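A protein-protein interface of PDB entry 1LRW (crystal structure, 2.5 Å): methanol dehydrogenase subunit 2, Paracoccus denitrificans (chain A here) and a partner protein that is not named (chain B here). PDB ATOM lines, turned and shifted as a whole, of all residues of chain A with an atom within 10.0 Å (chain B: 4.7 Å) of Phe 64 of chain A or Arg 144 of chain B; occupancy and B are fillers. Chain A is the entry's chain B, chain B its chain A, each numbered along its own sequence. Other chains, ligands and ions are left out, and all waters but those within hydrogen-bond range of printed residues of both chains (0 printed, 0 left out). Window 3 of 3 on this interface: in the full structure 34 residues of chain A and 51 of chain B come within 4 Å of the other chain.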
ATOM      1  N   ARG A  50       9.715 -39.789  -3.973  1.00  0.00           N
ATOM      2  CA  ARG A  50       8.846 -38.654  -3.669  1.00  0.00           C
ATOM      3  C   ARG A  50       9.584 -37.537  -2.938  1.00  0.00           C
ATOM      4  O   ARG A  50       9.310 -36.355  -3.147  1.00  0.00           O
ATOM      5  CB  ARG A  50       7.641 -39.100  -2.830  1.00  0.00           C
ATOM      6  CG  ARG A  50       6.577 -39.852  -3.617  1.00  0.00           C
ATOM      7  CD  ARG A  50       5.198 -39.725  -2.971  1.00  0.00           C
ATOM      8  NE  ARG A  50       5.035 -40.590  -1.808  1.00  0.00           N
ATOM      9  CZ  ARG A  50       4.891 -41.910  -1.870  1.00  0.00           C
ATOM     10  NH1 ARG A  50       4.746 -42.621  -0.758  1.00  0.00           N
ATOM     11  NH2 ARG A  50       4.881 -42.521  -3.043  1.00  0.00           N
ATOM     12  N   ASN A  51      10.517 -37.918  -2.073  1.00  0.00           N
ATOM     13  CA  ASN A  51      11.302 -36.956  -1.315  1.00  0.00           C
ATOM     14  C   ASN A  51      12.144 -36.089  -2.231  1.00  0.00           C
ATOM     15  O   ASN A  51      12.308 -34.899  -1.983  1.00  0.00           O
ATOM     16  CB  ASN A  51      12.208 -37.680  -0.318  1.00  0.00           C
ATOM     17  CG  ASN A  51      11.479 -38.072   0.951  1.00  0.00           C
ATOM     18  OD1 ASN A  51      11.913 -38.960   1.678  1.00  0.00           O
ATOM     19  ND2 ASN A  51      10.374 -37.399   1.230  1.00  0.00           N
ATOM     20  N   GLU A  52      12.679 -36.687  -3.290  1.00  0.00           N
ATOM     21  CA  GLU A  52      13.504 -35.941  -4.235  1.00  0.00           C
ATOM     22  C   GLU A  52      12.688 -34.825  -4.855  1.00  0.00           C
ATOM     23  O   GLU A  52      13.176 -33.707  -5.056  1.00  0.00           O
ATOM     24  CB  GLU A  52      14.029 -36.852  -5.341  1.00  0.00           C
ATOM     25  CG  GLU A  52      14.907 -37.976  -4.853  1.00  0.00           C
ATOM     26  CD  GLU A  52      15.731 -38.585  -5.965  1.00  0.00           C
ATOM     27  OE1 GLU A  52      16.341 -39.653  -5.727  1.00  0.00           O
ATOM     28  OE2 GLU A  52      15.777 -37.990  -7.069  1.00  0.00           O
ATOM     29  N   TRP A  53      11.434 -35.135  -5.161  1.00  0.00           N
ATOM     30  CA  TRP A  53      10.564 -34.145  -5.755  1.00  0.00           C
ATOM     31  C   TRP A  53      10.256 -33.045  -4.761  1.00  0.00           C
ATOM     32  O   TRP A  53      10.240 -31.865  -5.119  1.00  0.00           O
ATOM     33  CB  TRP A  53       9.285 -34.807  -6.266  1.00  0.00           C
ATOM     34  CG  TRP A  53       9.491 -35.432  -7.609  1.00  0.00           C
ATOM     35  CD1 TRP A  53       9.753 -36.745  -7.877  1.00  0.00           C
ATOM     36  CD2 TRP A  53       9.541 -34.748  -8.865  1.00  0.00           C
ATOM     37  NE1 TRP A  53       9.966 -36.921  -9.226  1.00  0.00           N
ATOM     38  CE2 TRP A  53       9.843 -35.709  -9.856  1.00  0.00           C
ATOM     39  CE3 TRP A  53       9.361 -33.410  -9.252  1.00  0.00           C
ATOM     40  CZ2 TRP A  53       9.972 -35.377 -11.209  1.00  0.00           C
ATOM     41  CZ3 TRP A  53       9.490 -33.078 -10.600  1.00  0.00           C
ATOM     42  CH2 TRP A  53       9.793 -34.060 -11.560  1.00  0.00           C
ATOM     43  N   ARG A  54      10.040 -33.434  -3.507  1.00  0.00           N
ATOM     44  CA  ARG A  54       9.751 -32.474  -2.450  1.00  0.00           C
ATOM     45  C   ARG A  54      10.945 -31.543  -2.272  1.00  0.00           C
ATOM     46  O   ARG A  54      10.791 -30.321  -2.180  1.00  0.00           O
ATOM     47  CB  ARG A  54       9.463 -33.193  -1.130  1.00  0.00           C
ATOM     48  CG  ARG A  54       8.308 -34.168  -1.201  1.00  0.00           C
ATOM     49  CD  ARG A  54       7.710 -34.438   0.174  1.00  0.00           C
ATOM     50  NE  ARG A  54       6.576 -35.354   0.090  1.00  0.00           N
ATOM     51  CZ  ARG A  54       6.684 -36.679   0.083  1.00  0.00           C
ATOM     52  NH1 ARG A  54       5.599 -37.437  -0.010  1.00  0.00           N
ATOM     53  NH2 ARG A  54       7.878 -37.246   0.191  1.00  0.00           N
ATOM     54  N   VAL A  55      12.136 -32.125  -2.232  1.00  0.00           N
ATOM     55  CA  VAL A  55      13.350 -31.340  -2.061  1.00  0.00           C
ATOM     56  C   VAL A  55      13.551 -30.397  -3.236  1.00  0.00           C
ATOM     57  O   VAL A  55      13.862 -29.218  -3.051  1.00  0.00           O
ATOM     58  CB  VAL A  55      14.595 -32.238  -1.933  1.00  0.00           C
ATOM     59  CG1 VAL A  55      15.842 -31.379  -1.882  1.00  0.00           C
ATOM     60  CG2 VAL A  55      14.498 -33.091  -0.679  1.00  0.00           C
ATOM     61  N   TRP A  56      13.372 -30.927  -4.444  1.00  0.00           N
ATOM     62  CA  TRP A  56      13.540 -30.142  -5.659  1.00  0.00           C
ATOM     63  C   TRP A  56      12.575 -28.964  -5.734  1.00  0.00           C
ATOM     64  O   TRP A  56      12.976 -27.844  -6.047  1.00  0.00           O
ATOM     65  CB  TRP A  56      13.347 -31.023  -6.897  1.00  0.00           C
ATOM     66  CG  TRP A  56      13.415 -30.254  -8.187  1.00  0.00           C
ATOM     67  CD1 TRP A  56      14.535 -29.746  -8.785  1.00  0.00           C
ATOM     68  CD2 TRP A  56      12.310 -29.866  -9.014  1.00  0.00           C
ATOM     69  NE1 TRP A  56      14.196 -29.064  -9.932  1.00  0.00           N
ATOM     70  CE2 TRP A  56      12.838 -29.122 -10.095  1.00  0.00           C
ATOM     71  CE3 TRP A  56      10.925 -30.072  -8.944  1.00  0.00           C
ATOM     72  CZ2 TRP A  56      12.026 -28.582 -11.102  1.00  0.00           C
ATOM     73  CZ3 TRP A  56      10.117 -29.534  -9.947  1.00  0.00           C
ATOM     74  CH2 TRP A  56      10.673 -28.798 -11.012  1.00  0.00           C
ATOM     75  N   ASN A  57      11.306 -29.215  -5.444  1.00  0.00           N
ATOM     76  CA  ASN A  57      10.309 -28.158  -5.517  1.00  0.00           C
ATOM     77  C   ASN A  57      10.520 -26.992  -4.545  1.00  0.00           C
ATOM     78  O   ASN A  57      10.265 -25.843  -4.898  1.00  0.00           O
ATOM     79  CB  ASN A  57       8.908 -28.744  -5.336  1.00  0.00           C
ATOM     80  CG  ASN A  57       7.829 -27.694  -5.447  1.00  0.00           C
ATOM     81  OD1 ASN A  57       7.505 -27.006  -4.476  1.00  0.00           O
ATOM     82  ND2 ASN A  57       7.277 -27.547  -6.642  1.00  0.00           N
ATOM     83  N   MET A  58      10.976 -27.267  -3.326  1.00  0.00           N
ATOM     84  CA  MET A  58      11.191 -26.177  -2.385  1.00  0.00           C
ATOM     85  C   MET A  58      12.381 -25.335  -2.821  1.00  0.00           C
ATOM     86  O   MET A  58      12.414 -24.126  -2.589  1.00  0.00           O
ATOM     87  CB  MET A  58      11.428 -26.698  -0.966  1.00  0.00           C
ATOM     88  CG  MET A  58      11.797 -25.587   0.013  1.00  0.00           C
ATOM     89  SD  MET A  58      11.790 -26.065   1.742  1.00  0.00           S
ATOM     90  CE  MET A  58      13.164 -27.218   1.763  1.00  0.00           C
ATOM     91  N   LYS A  59      13.355 -25.977  -3.460  1.00  0.00           N
ATOM     92  CA  LYS A  59      14.549 -25.282  -3.919  1.00  0.00           C
ATOM     93  C   LYS A  59      14.249 -24.374  -5.106  1.00  0.00           C
ATOM     94  O   LYS A  59      14.777 -23.269  -5.206  1.00  0.00           O
ATOM     95  CB  LYS A  59      15.634 -26.292  -4.301  1.00  0.00           C
ATOM     96  CG  LYS A  59      16.952 -25.645  -4.695  1.00  0.00           C
ATOM     97  CD  LYS A  59      18.082 -26.663  -4.789  1.00  0.00           C
ATOM     98  CE  LYS A  59      19.424 -25.977  -5.039  1.00  0.00           C
ATOM     99  NZ  LYS A  59      20.571 -26.934  -5.025  1.00  0.00           N
ATOM    100  N   LYS A  60      13.391 -24.844  -6.002  1.00  0.00           N
ATOM    101  CA  LYS A  60      13.029 -24.068  -7.175  1.00  0.00           C
ATOM    102  C   LYS A  60      11.970 -23.002  -6.871  1.00  0.00           C
ATOM    103  O   LYS A  60      12.063 -21.872  -7.351  1.00  0.00           O
ATOM    104  CB  LYS A  60      12.529 -25.010  -8.278  1.00  0.00           C
ATOM    105  CG  LYS A  60      12.278 -24.324  -9.612  1.00  0.00           C
ATOM    106  CD  LYS A  60      11.967 -25.328 -10.708  1.00  0.00           C
ATOM    107  CE  LYS A  60      11.767 -24.639 -12.056  1.00  0.00           C
ATOM    108  NZ  LYS A  60      11.538 -25.610 -13.171  1.00  0.00           N
ATOM    109  N   THR A  61      10.975 -23.361  -6.064  1.00  0.00           N
ATOM    110  CA  THR A  61       9.890 -22.447  -5.710  1.00  0.00           C
ATOM    111  C   THR A  61      10.250 -21.480  -4.601  1.00  0.00           C
ATOM    112  O   THR A  61      10.029 -20.280  -4.726  1.00  0.00           O
ATOM    113  CB  THR A  61       8.634 -23.207  -5.256  1.00  0.00           C
ATOM    114  OG1 THR A  61       8.223 -24.118  -6.279  1.00  0.00           O
ATOM    115  CG2 THR A  61       7.506 -22.239  -4.990  1.00  0.00           C
ATOM    116  N   GLY A  62      10.792 -22.006  -3.508  1.00  0.00           N
ATOM    117  CA  GLY A  62      11.152 -21.166  -2.381  1.00  0.00           C
ATOM    118  C   GLY A  62      10.251 -21.483  -1.205  1.00  0.00           C
ATOM    119  O   GLY A  62      10.524 -21.103  -0.065  1.00  0.00           O
ATOM    120  N   LYS A  63       9.160 -22.182  -1.498  1.00  0.00           N
ATOM    121  CA  LYS A  63       8.191 -22.588  -0.485  1.00  0.00           C
ATOM    122  C   LYS A  63       8.134 -24.116  -0.508  1.00  0.00           C
ATOM    123  O   LYS A  63       8.438 -24.745  -1.525  1.00  0.00           O
ATOM    124  CB  LYS A  63       6.803 -22.006  -0.792  1.00  0.00           C
ATOM    125  CG  LYS A  63       6.141 -22.624  -2.013  1.00  0.00           C
ATOM    126  CD  LYS A  63       4.771 -22.035  -2.309  1.00  0.00           C
ATOM    127  CE  LYS A  63       4.161 -22.692  -3.551  1.00  0.00           C
ATOM    128  NZ  LYS A  63       2.827 -22.123  -3.914  1.00  0.00           N
ATOM    129  N   PHE A  64       7.735 -24.708   0.610  1.00  0.00           N
ATOM    130  CA  PHE A  64       7.672 -26.156   0.704  1.00  0.00           C
ATOM    131  C   PHE A  64       6.295 -26.733   0.394  1.00  0.00           C
ATOM    132  O   PHE A  64       5.265 -26.132   0.708  1.00  0.00           O
ATOM    133  CB  PHE A  64       8.108 -26.600   2.102  1.00  0.00           C
ATOM    134  CG  PHE A  64       8.130 -28.081   2.276  1.00  0.00           C
ATOM    135  CD1 PHE A  64       9.163 -28.835   1.744  1.00  0.00           C
ATOM    136  CD2 PHE A  64       7.090 -28.728   2.929  1.00  0.00           C
ATOM    137  CE1 PHE A  64       9.155 -30.218   1.858  1.00  0.00           C
ATOM    138  CE2 PHE A  64       7.070 -30.103   3.048  1.00  0.00           C
ATOM    139  CZ  PHE A  64       8.102 -30.852   2.513  1.00  0.00           C
ATOM    140  N   GLU A  65       6.295 -27.909  -0.226  1.00  0.00           N
ATOM    141  CA  GLU A  65       5.067 -28.609  -0.578  1.00  0.00           C
ATOM    142  C   GLU A  65       5.270 -30.108  -0.356  1.00  0.00           C
ATOM    143  O   GLU A  65       6.165 -30.717  -0.937  1.00  0.00           O
ATOM    144  CB  GLU A  65       4.695 -28.335  -2.037  1.00  0.00           C
ATOM    145  CG  GLU A  65       3.430 -29.033  -2.495  1.00  0.00           C
ATOM    146  CD  GLU A  65       2.282 -28.825  -1.533  1.00  0.00           C
ATOM    147  OE1 GLU A  65       2.044 -27.660  -1.156  1.00  0.00           O
ATOM    148  OE2 GLU A  65       1.617 -29.815  -1.156  1.00  0.00           O
ATOM    149  N   TYR A  66       4.436 -30.696   0.495  1.00  0.00           N
ATOM    150  CA  TYR A  66       4.545 -32.113   0.801  1.00  0.00           C
ATOM    151  C   TYR A  66       3.860 -33.005  -0.225  1.00  0.00           C
ATOM    152  O   TYR A  66       4.396 -34.041  -0.606  1.00  0.00           O
ATOM    153  CB  TYR A  66       3.960 -32.400   2.187  1.00  0.00           C
ATOM    154  CG  TYR A  66       3.828 -33.878   2.484  1.00  0.00           C
ATOM    155  CD1 TYR A  66       4.891 -34.605   3.023  1.00  0.00           C
ATOM    156  CD2 TYR A  66       2.655 -34.562   2.172  1.00  0.00           C
ATOM    157  CE1 TYR A  66       4.784 -35.979   3.240  1.00  0.00           C
ATOM    158  CE2 TYR A  66       2.539 -35.932   2.384  1.00  0.00           C
ATOM    159  CZ  TYR A  66       3.602 -36.635   2.915  1.00  0.00           C
ATOM    160  OH  TYR A  66       3.476 -37.989   3.102  1.00  0.00           O
ATOM    161  N   ASP A  67       2.667 -32.604  -0.650  1.00  0.00           N
ATOM    162  CA  ASP A  67       1.891 -33.369  -1.620  1.00  0.00           C
ATOM    163  C   ASP A  67       2.510 -33.231  -3.006  1.00  0.00           C
ATOM    164  O   ASP A  67       2.361 -32.193  -3.655  1.00  0.00           O
ATOM    165  CB  ASP A  67       0.454 -32.853  -1.661  1.00  0.00           C
ATOM    166  CG  ASP A  67      -0.510 -33.848  -2.283  1.00  0.00           C
ATOM    167  OD1 ASP A  67      -0.091 -34.611  -3.182  1.00  0.00           O
ATOM    168  OD2 ASP A  67      -1.696 -33.857  -1.878  1.00  0.00           O
ATOM    169  N   VAL A  68       3.200 -34.278  -3.454  1.00  0.00           N
ATOM    170  CA  VAL A  68       3.853 -34.273  -4.762  1.00  0.00           C
ATOM    171  C   VAL A  68       2.852 -34.038  -5.894  1.00  0.00           C
ATOM    172  O   VAL A  68       3.202 -33.488  -6.940  1.00  0.00           O
ATOM    173  CB  VAL A  68       4.606 -35.609  -5.013  1.00  0.00           C
ATOM    174  CG1 VAL A  68       5.725 -35.775  -3.995  1.00  0.00           C
ATOM    175  CG2 VAL A  68       3.641 -36.788  -4.930  1.00  0.00           C
ATOM    176  N   LYS A  70       0.687 -31.932  -6.074  1.00  0.00           N
ATOM    177  CA  LYS A  70       0.518 -30.504  -6.284  1.00  0.00           C
ATOM    178  C   LYS A  70       1.827 -29.823  -6.658  1.00  0.00           C
ATOM    179  O   LYS A  70       1.932 -28.600  -6.608  1.00  0.00           O
ATOM    180  CB  LYS A  70      -0.060 -29.855  -5.026  1.00  0.00           C
ATOM    181  CG  LYS A  70      -1.443 -30.361  -4.653  1.00  0.00           C
ATOM    182  CD  LYS A  70      -1.947 -29.713  -3.371  1.00  0.00           C
ATOM    183  CE  LYS A  70      -2.056 -28.201  -3.512  1.00  0.00           C
ATOM    184  NZ  LYS A  70      -2.453 -27.542  -2.233  1.00  0.00           N
ATOM    185  N   ILE A  71       2.830 -30.607  -7.028  1.00  0.00           N
ATOM    186  CA  ILE A  71       4.112 -30.030  -7.412  1.00  0.00           C
ATOM    187  C   ILE A  71       4.142 -29.817  -8.916  1.00  0.00           C
ATOM    188  O   ILE A  71       4.013 -30.764  -9.698  1.00  0.00           O
ATOM    189  CB  ILE A  71       5.289 -30.936  -6.993  1.00  0.00           C
ATOM    190  CG1 ILE A  71       5.440 -30.903  -5.473  1.00  0.00           C
ATOM    191  CG2 ILE A  71       6.574 -30.479  -7.664  1.00  0.00           C
ATOM    192  CD1 ILE A  71       6.473 -31.866  -4.940  1.00  0.00           C
ATOM    193  N   VAL B 120      19.184 -19.624   8.615  1.00  0.00           N
ATOM    194  CA  VAL B 120      17.990 -20.300   9.096  1.00  0.00           C
ATOM    195  C   VAL B 120      17.966 -20.310  10.615  1.00  0.00           C
ATOM    196  O   VAL B 120      18.888 -20.810  11.256  1.00  0.00           O
ATOM    197  CB  VAL B 120      17.935 -21.749   8.610  1.00  0.00           C
ATOM    198  CG1 VAL B 120      16.672 -22.410   9.130  1.00  0.00           C
ATOM    199  CG2 VAL B 120      17.981 -21.791   7.094  1.00  0.00           C
ATOM    200  N   LEU B 123      15.680 -24.603  14.822  1.00  0.00           N
ATOM    201  CA  LEU B 123      14.620 -25.516  14.422  1.00  0.00           C
ATOM    202  C   LEU B 123      14.423 -26.619  15.440  1.00  0.00           C
ATOM    203  O   LEU B 123      15.369 -27.036  16.114  1.00  0.00           O
ATOM    204  CB  LEU B 123      14.944 -26.166  13.081  1.00  0.00           C
ATOM    205  CG  LEU B 123      14.962 -25.317  11.819  1.00  0.00           C
ATOM    206  CD1 LEU B 123      15.389 -26.191  10.656  1.00  0.00           C
ATOM    207  CD2 LEU B 123      13.589 -24.728  11.563  1.00  0.00           C
ATOM    208  N   ALA B 135      10.574 -30.821  10.370  1.00  0.00           N
ATOM    209  CA  ALA B 135      11.299 -29.704  10.961  1.00  0.00           C
ATOM    210  C   ALA B 135      10.340 -28.535  11.121  1.00  0.00           C
ATOM    211  O   ALA B 135       9.479 -28.305  10.276  1.00  0.00           O
ATOM    212  CB  ALA B 135      12.470 -29.307  10.072  1.00  0.00           C
ATOM    213  N   MET B 136      10.486 -27.799  12.215  1.00  0.00           N
ATOM    214  CA  MET B 136       9.617 -26.663  12.472  1.00  0.00           C
ATOM    215  C   MET B 136      10.435 -25.544  13.074  1.00  0.00           C
ATOM    216  O   MET B 136      11.390 -25.784  13.811  1.00  0.00           O
ATOM    217  CB  MET B 136       8.516 -27.037  13.465  1.00  0.00           C
ATOM    218  CG  MET B 136       7.918 -28.413  13.270  1.00  0.00           C
ATOM    219  SD  MET B 136       7.041 -28.972  14.755  1.00  0.00           S
ATOM    220  CE  MET B 136       8.370 -29.043  15.905  1.00  0.00           C
ATOM    221  N   GLU B 142       5.943 -23.197  13.023  1.00  0.00           N
ATOM    222  CA  GLU B 142       5.445 -23.525  11.698  1.00  0.00           C
ATOM    223  C   GLU B 142       6.397 -24.463  10.976  1.00  0.00           C
ATOM    224  O   GLU B 142       7.611 -24.300  11.021  1.00  0.00           O
ATOM    225  CB  GLU B 142       5.193 -22.258  10.886  1.00  0.00           C
ATOM    226  CG  GLU B 142       6.362 -21.316  10.801  1.00  0.00           C
ATOM    227  CD  GLU B 142       6.004 -20.020  10.086  1.00  0.00           C
ATOM    228  OE1 GLU B 142       5.476 -20.100   8.949  1.00  0.00           O
ATOM    229  OE2 GLU B 142       6.251 -18.929  10.655  1.00  0.00           O
ATOM    230  N   THR B 143       5.819 -25.457  10.315  1.00  0.00           N
ATOM    231  CA  THR B 143       6.566 -26.478   9.600  1.00  0.00           C
ATOM    232  C   THR B 143       7.473 -25.947   8.495  1.00  0.00           C
ATOM    233  O   THR B 143       7.061 -25.116   7.692  1.00  0.00           O
ATOM    234  CB  THR B 143       5.597 -27.516   8.996  1.00  0.00           C
ATOM    235  OG1 THR B 143       4.716 -28.000  10.019  1.00  0.00           O
ATOM    236  CG2 THR B 143       6.366 -28.685   8.406  1.00  0.00           C
ATOM    237  N   ARG B 144       8.710 -26.434   8.460  1.00  0.00           N
ATOM    238  CA  ARG B 144       9.662 -26.025   7.432  1.00  0.00           C
ATOM    239  C   ARG B 144       9.661 -27.080   6.329  1.00  0.00           C
ATOM    240  O   ARG B 144       9.594 -26.761   5.145  1.00  0.00           O
ATOM    241  CB  ARG B 144      11.066 -25.893   8.018  1.00  0.00           C
ATOM    242  CG  ARG B 144      12.102 -25.456   7.002  1.00  0.00           C
ATOM    243  CD  ARG B 144      13.475 -25.349   7.624  1.00  0.00           C
ATOM    244  NE  ARG B 144      14.165 -24.148   7.160  1.00  0.00           N
ATOM    245  CZ  ARG B 144      14.608 -23.964   5.922  1.00  0.00           C
ATOM    246  NH1 ARG B 144      15.216 -22.830   5.598  1.00  0.00           N
ATOM    247  NH2 ARG B 144      14.458 -24.917   5.014  1.00  0.00           N
ATOM    248  N   TRP B 145       9.751 -28.342   6.728  1.00  0.00           N
ATOM    249  CA  TRP B 145       9.728 -29.436   5.773  1.00  0.00           C
ATOM    250  C   TRP B 145       9.323 -30.748   6.426  1.00  0.00           C
ATOM    251  O   TRP B 145       9.336 -30.887   7.651  1.00  0.00           O
ATOM    252  CB  TRP B 145      11.088 -29.598   5.072  1.00  0.00           C
ATOM    253  CG  TRP B 145      12.291 -29.736   5.969  1.00  0.00           C
ATOM    254  CD1 TRP B 145      13.110 -28.730   6.412  1.00  0.00           C
ATOM    255  CD2 TRP B 145      12.836 -30.954   6.497  1.00  0.00           C
ATOM    256  NE1 TRP B 145      14.131 -29.248   7.177  1.00  0.00           N
ATOM    257  CE2 TRP B 145      13.987 -30.610   7.246  1.00  0.00           C
ATOM    258  CE3 TRP B 145      12.464 -32.302   6.410  1.00  0.00           C
ATOM    259  CZ2 TRP B 145      14.768 -31.568   7.902  1.00  0.00           C
ATOM    260  CZ3 TRP B 145      13.244 -33.255   7.064  1.00  0.00           C
ATOM    261  CH2 TRP B 145      14.382 -32.881   7.799  1.00  0.00           C
ATOM    262  N   ILE B 146       8.950 -31.705   5.588  1.00  0.00           N
ATOM    263  CA  ILE B 146       8.535 -33.024   6.040  1.00  0.00           C
ATOM    264  C   ILE B 146       9.051 -34.011   5.008  1.00  0.00           C
ATOM    265  O   ILE B 146       9.016 -33.731   3.815  1.00  0.00           O
ATOM    266  CB  ILE B 146       6.999 -33.149   6.087  1.00  0.00           C
ATOM    267  CG1 ILE B 146       6.403 -32.003   6.900  1.00  0.00           C
ATOM    268  CG2 ILE B 146       6.602 -34.491   6.681  1.00  0.00           C
ATOM    269  CD1 ILE B 146       4.888 -31.975   6.871  1.00  0.00           C
ATOM    270  N   MET B 147       9.536 -35.158   5.463  1.00  0.00           N
ATOM    271  CA  MET B 147      10.045 -36.180   4.561  1.00  0.00           C
ATOM    272  C   MET B 147       9.576 -37.545   5.058  1.00  0.00           C
ATOM    273  O   MET B 147       9.404 -37.741   6.266  1.00  0.00           O
ATOM    274  CB  MET B 147      11.571 -36.135   4.527  1.00  0.00           C
ATOM    275  CG  MET B 147      12.172 -34.841   3.979  1.00  0.00           C
ATOM    276  SD  MET B 147      12.015 -34.613   2.184  1.00  0.00           S
ATOM    277  CE  MET B 147      11.559 -32.923   2.137  1.00  0.00           C
ATOM    278  N   LYS B 190      18.538 -28.248   7.172  1.00  0.00           N
ATOM    279  CA  LYS B 190      17.855 -27.199   6.431  1.00  0.00           C
ATOM    280  C   LYS B 190      16.875 -27.663   5.354  1.00  0.00           C
ATOM    281  O   LYS B 190      15.716 -27.243   5.341  1.00  0.00           O
ATOM    282  CB  LYS B 190      18.879 -26.268   5.794  1.00  0.00           C
ATOM    283  CG  LYS B 190      19.779 -25.555   6.782  1.00  0.00           C
ATOM    284  CD  LYS B 190      20.836 -24.748   6.044  1.00  0.00           C
ATOM    285  CE  LYS B 190      21.789 -24.078   7.004  1.00  0.00           C
ATOM    286  NZ  LYS B 190      22.898 -23.406   6.281  1.00  0.00           N
ATOM    287  N   SER B 191      17.329 -28.532   4.457  1.00  0.00           N
ATOM    288  CA  SER B 191      16.482 -28.993   3.365  1.00  0.00           C
ATOM    289  C   SER B 191      15.781 -30.318   3.593  1.00  0.00           C
ATOM    290  O   SER B 191      14.792 -30.621   2.926  1.00  0.00           O
ATOM    291  CB  SER B 191      17.304 -29.102   2.084  1.00  0.00           C
ATOM    292  OG  SER B 191      18.260 -30.143   2.191  1.00  0.00           O
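The side-chain sulfur (SD) of Met 147 of chain B sits at hydrogen-bond distance from the side-chain amide nitrogen (ND2) of Asn 51 of chain A (3.4 Å).
The backbone carbonyl oxygen (O) of Ala 135 of chain B lies within hydrogen-bond range of the backbone NH (N) of Arg 144 of chain B.
The backbone carbonyl oxygen (O) of Trp 145 of chain B sits at hydrogen-bond distance from the backbone NH (N) of Ala 135 of chain B.
NH2 of Arg 144 of chain B sits at hydrogen-bond distance from O of Lys 190 of chain B (2.7 Å).
NE1 of Trp 145 of chain B lies within hydrogen-bond range of O of Lys 190 of chain B (3.1 Å).
The guanidinium group (NH2) of Arg 54 of chain A lies close to the side-chain amide nitrogen (ND2) of Asn 51 of chain A (2.7 Å).
The guanidinium group (NE) of Arg 54 of chain A is in hydrogen-bond range of the backbone carbonyl oxygen (O) of Tyr 66 of chain A.
Arg 54 of chain A touches Ile 146 of chain B.
Arg 54 of chain A touches Met 147 of chain B (CB to CE, 3.9 Å).
Ser 191 of chain B touches Met 58 of chain A (O to CE, 3.9 Å).
Phe 64 of chain A touches Arg 144 of chain B (CB to O, 3.4 Å).
CE1 of Phe 64 of chain A touches CB of Trp 145 of chain B, 3.8 Å away.
Phe 64 of chain A touches Ile 146 of chain B (CZ to O, 3.3 Å).
Phe 64 of chain A touches Met 147 of chain B (CE1 to CE, 3.6 Å).
CD1 of Tyr 66 of chain A touches CB of Ile 146 of chain B, 3.99 Å away.
Of chain B, only Arg 144, Trp 145, Ile 146 and Met 147 come within 4 Å of Phe 64 of chain A.
Of chain A, only Phe 64 (3.4 Å) comes within 4 Å of Arg 144 of chain B.
No residue of chain A comes within 4 Å of Ala 135 of chain B.
No residue of chain A comes within 4 Å of Thr 143 of chain B.
Printed residues of chain B within 4 Å of Arg 54 of chain A: Ile 146 (3.9 Å) and Met 147 (3.9 Å).
Printed residues of chain A within 4 Å of Trp 145 of chain B: Phe 64.
Of the printed residues of chain B, Met 58 of chain A touches Ser 191.
Printed residues of chain B within 4 Å of Tyr 66 of chain A: Ile 146 (3.99 Å).
Of the printed residues of chain A, Ser 191 of chain B touches Met 58.
Glu 52 of chain A touches none of the printed residues of chain B.
Asn 57 of chain A touches none of the printed residues of chain B.
The nearest printed residue of chain B that does not touch Phe 64 of chain A is Thr 143 of chain B (5.5 Å).
The nearest residue of chain A that does not touch Arg 144 of chain B is Met 58 of chain A (4.1 Å).
The nearest printed residue of chain A that does not touch Met 147 of chain B is Val 55 of chain A (4.1 Å).
Along chain A the printed residues that touch a printed residue of chain B span positions 51 to 66.
Printed residues of chain B that touch a printed residue of chain A: Arg 144, Trp 145, Ile 146, Met 147 and Ser 191.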
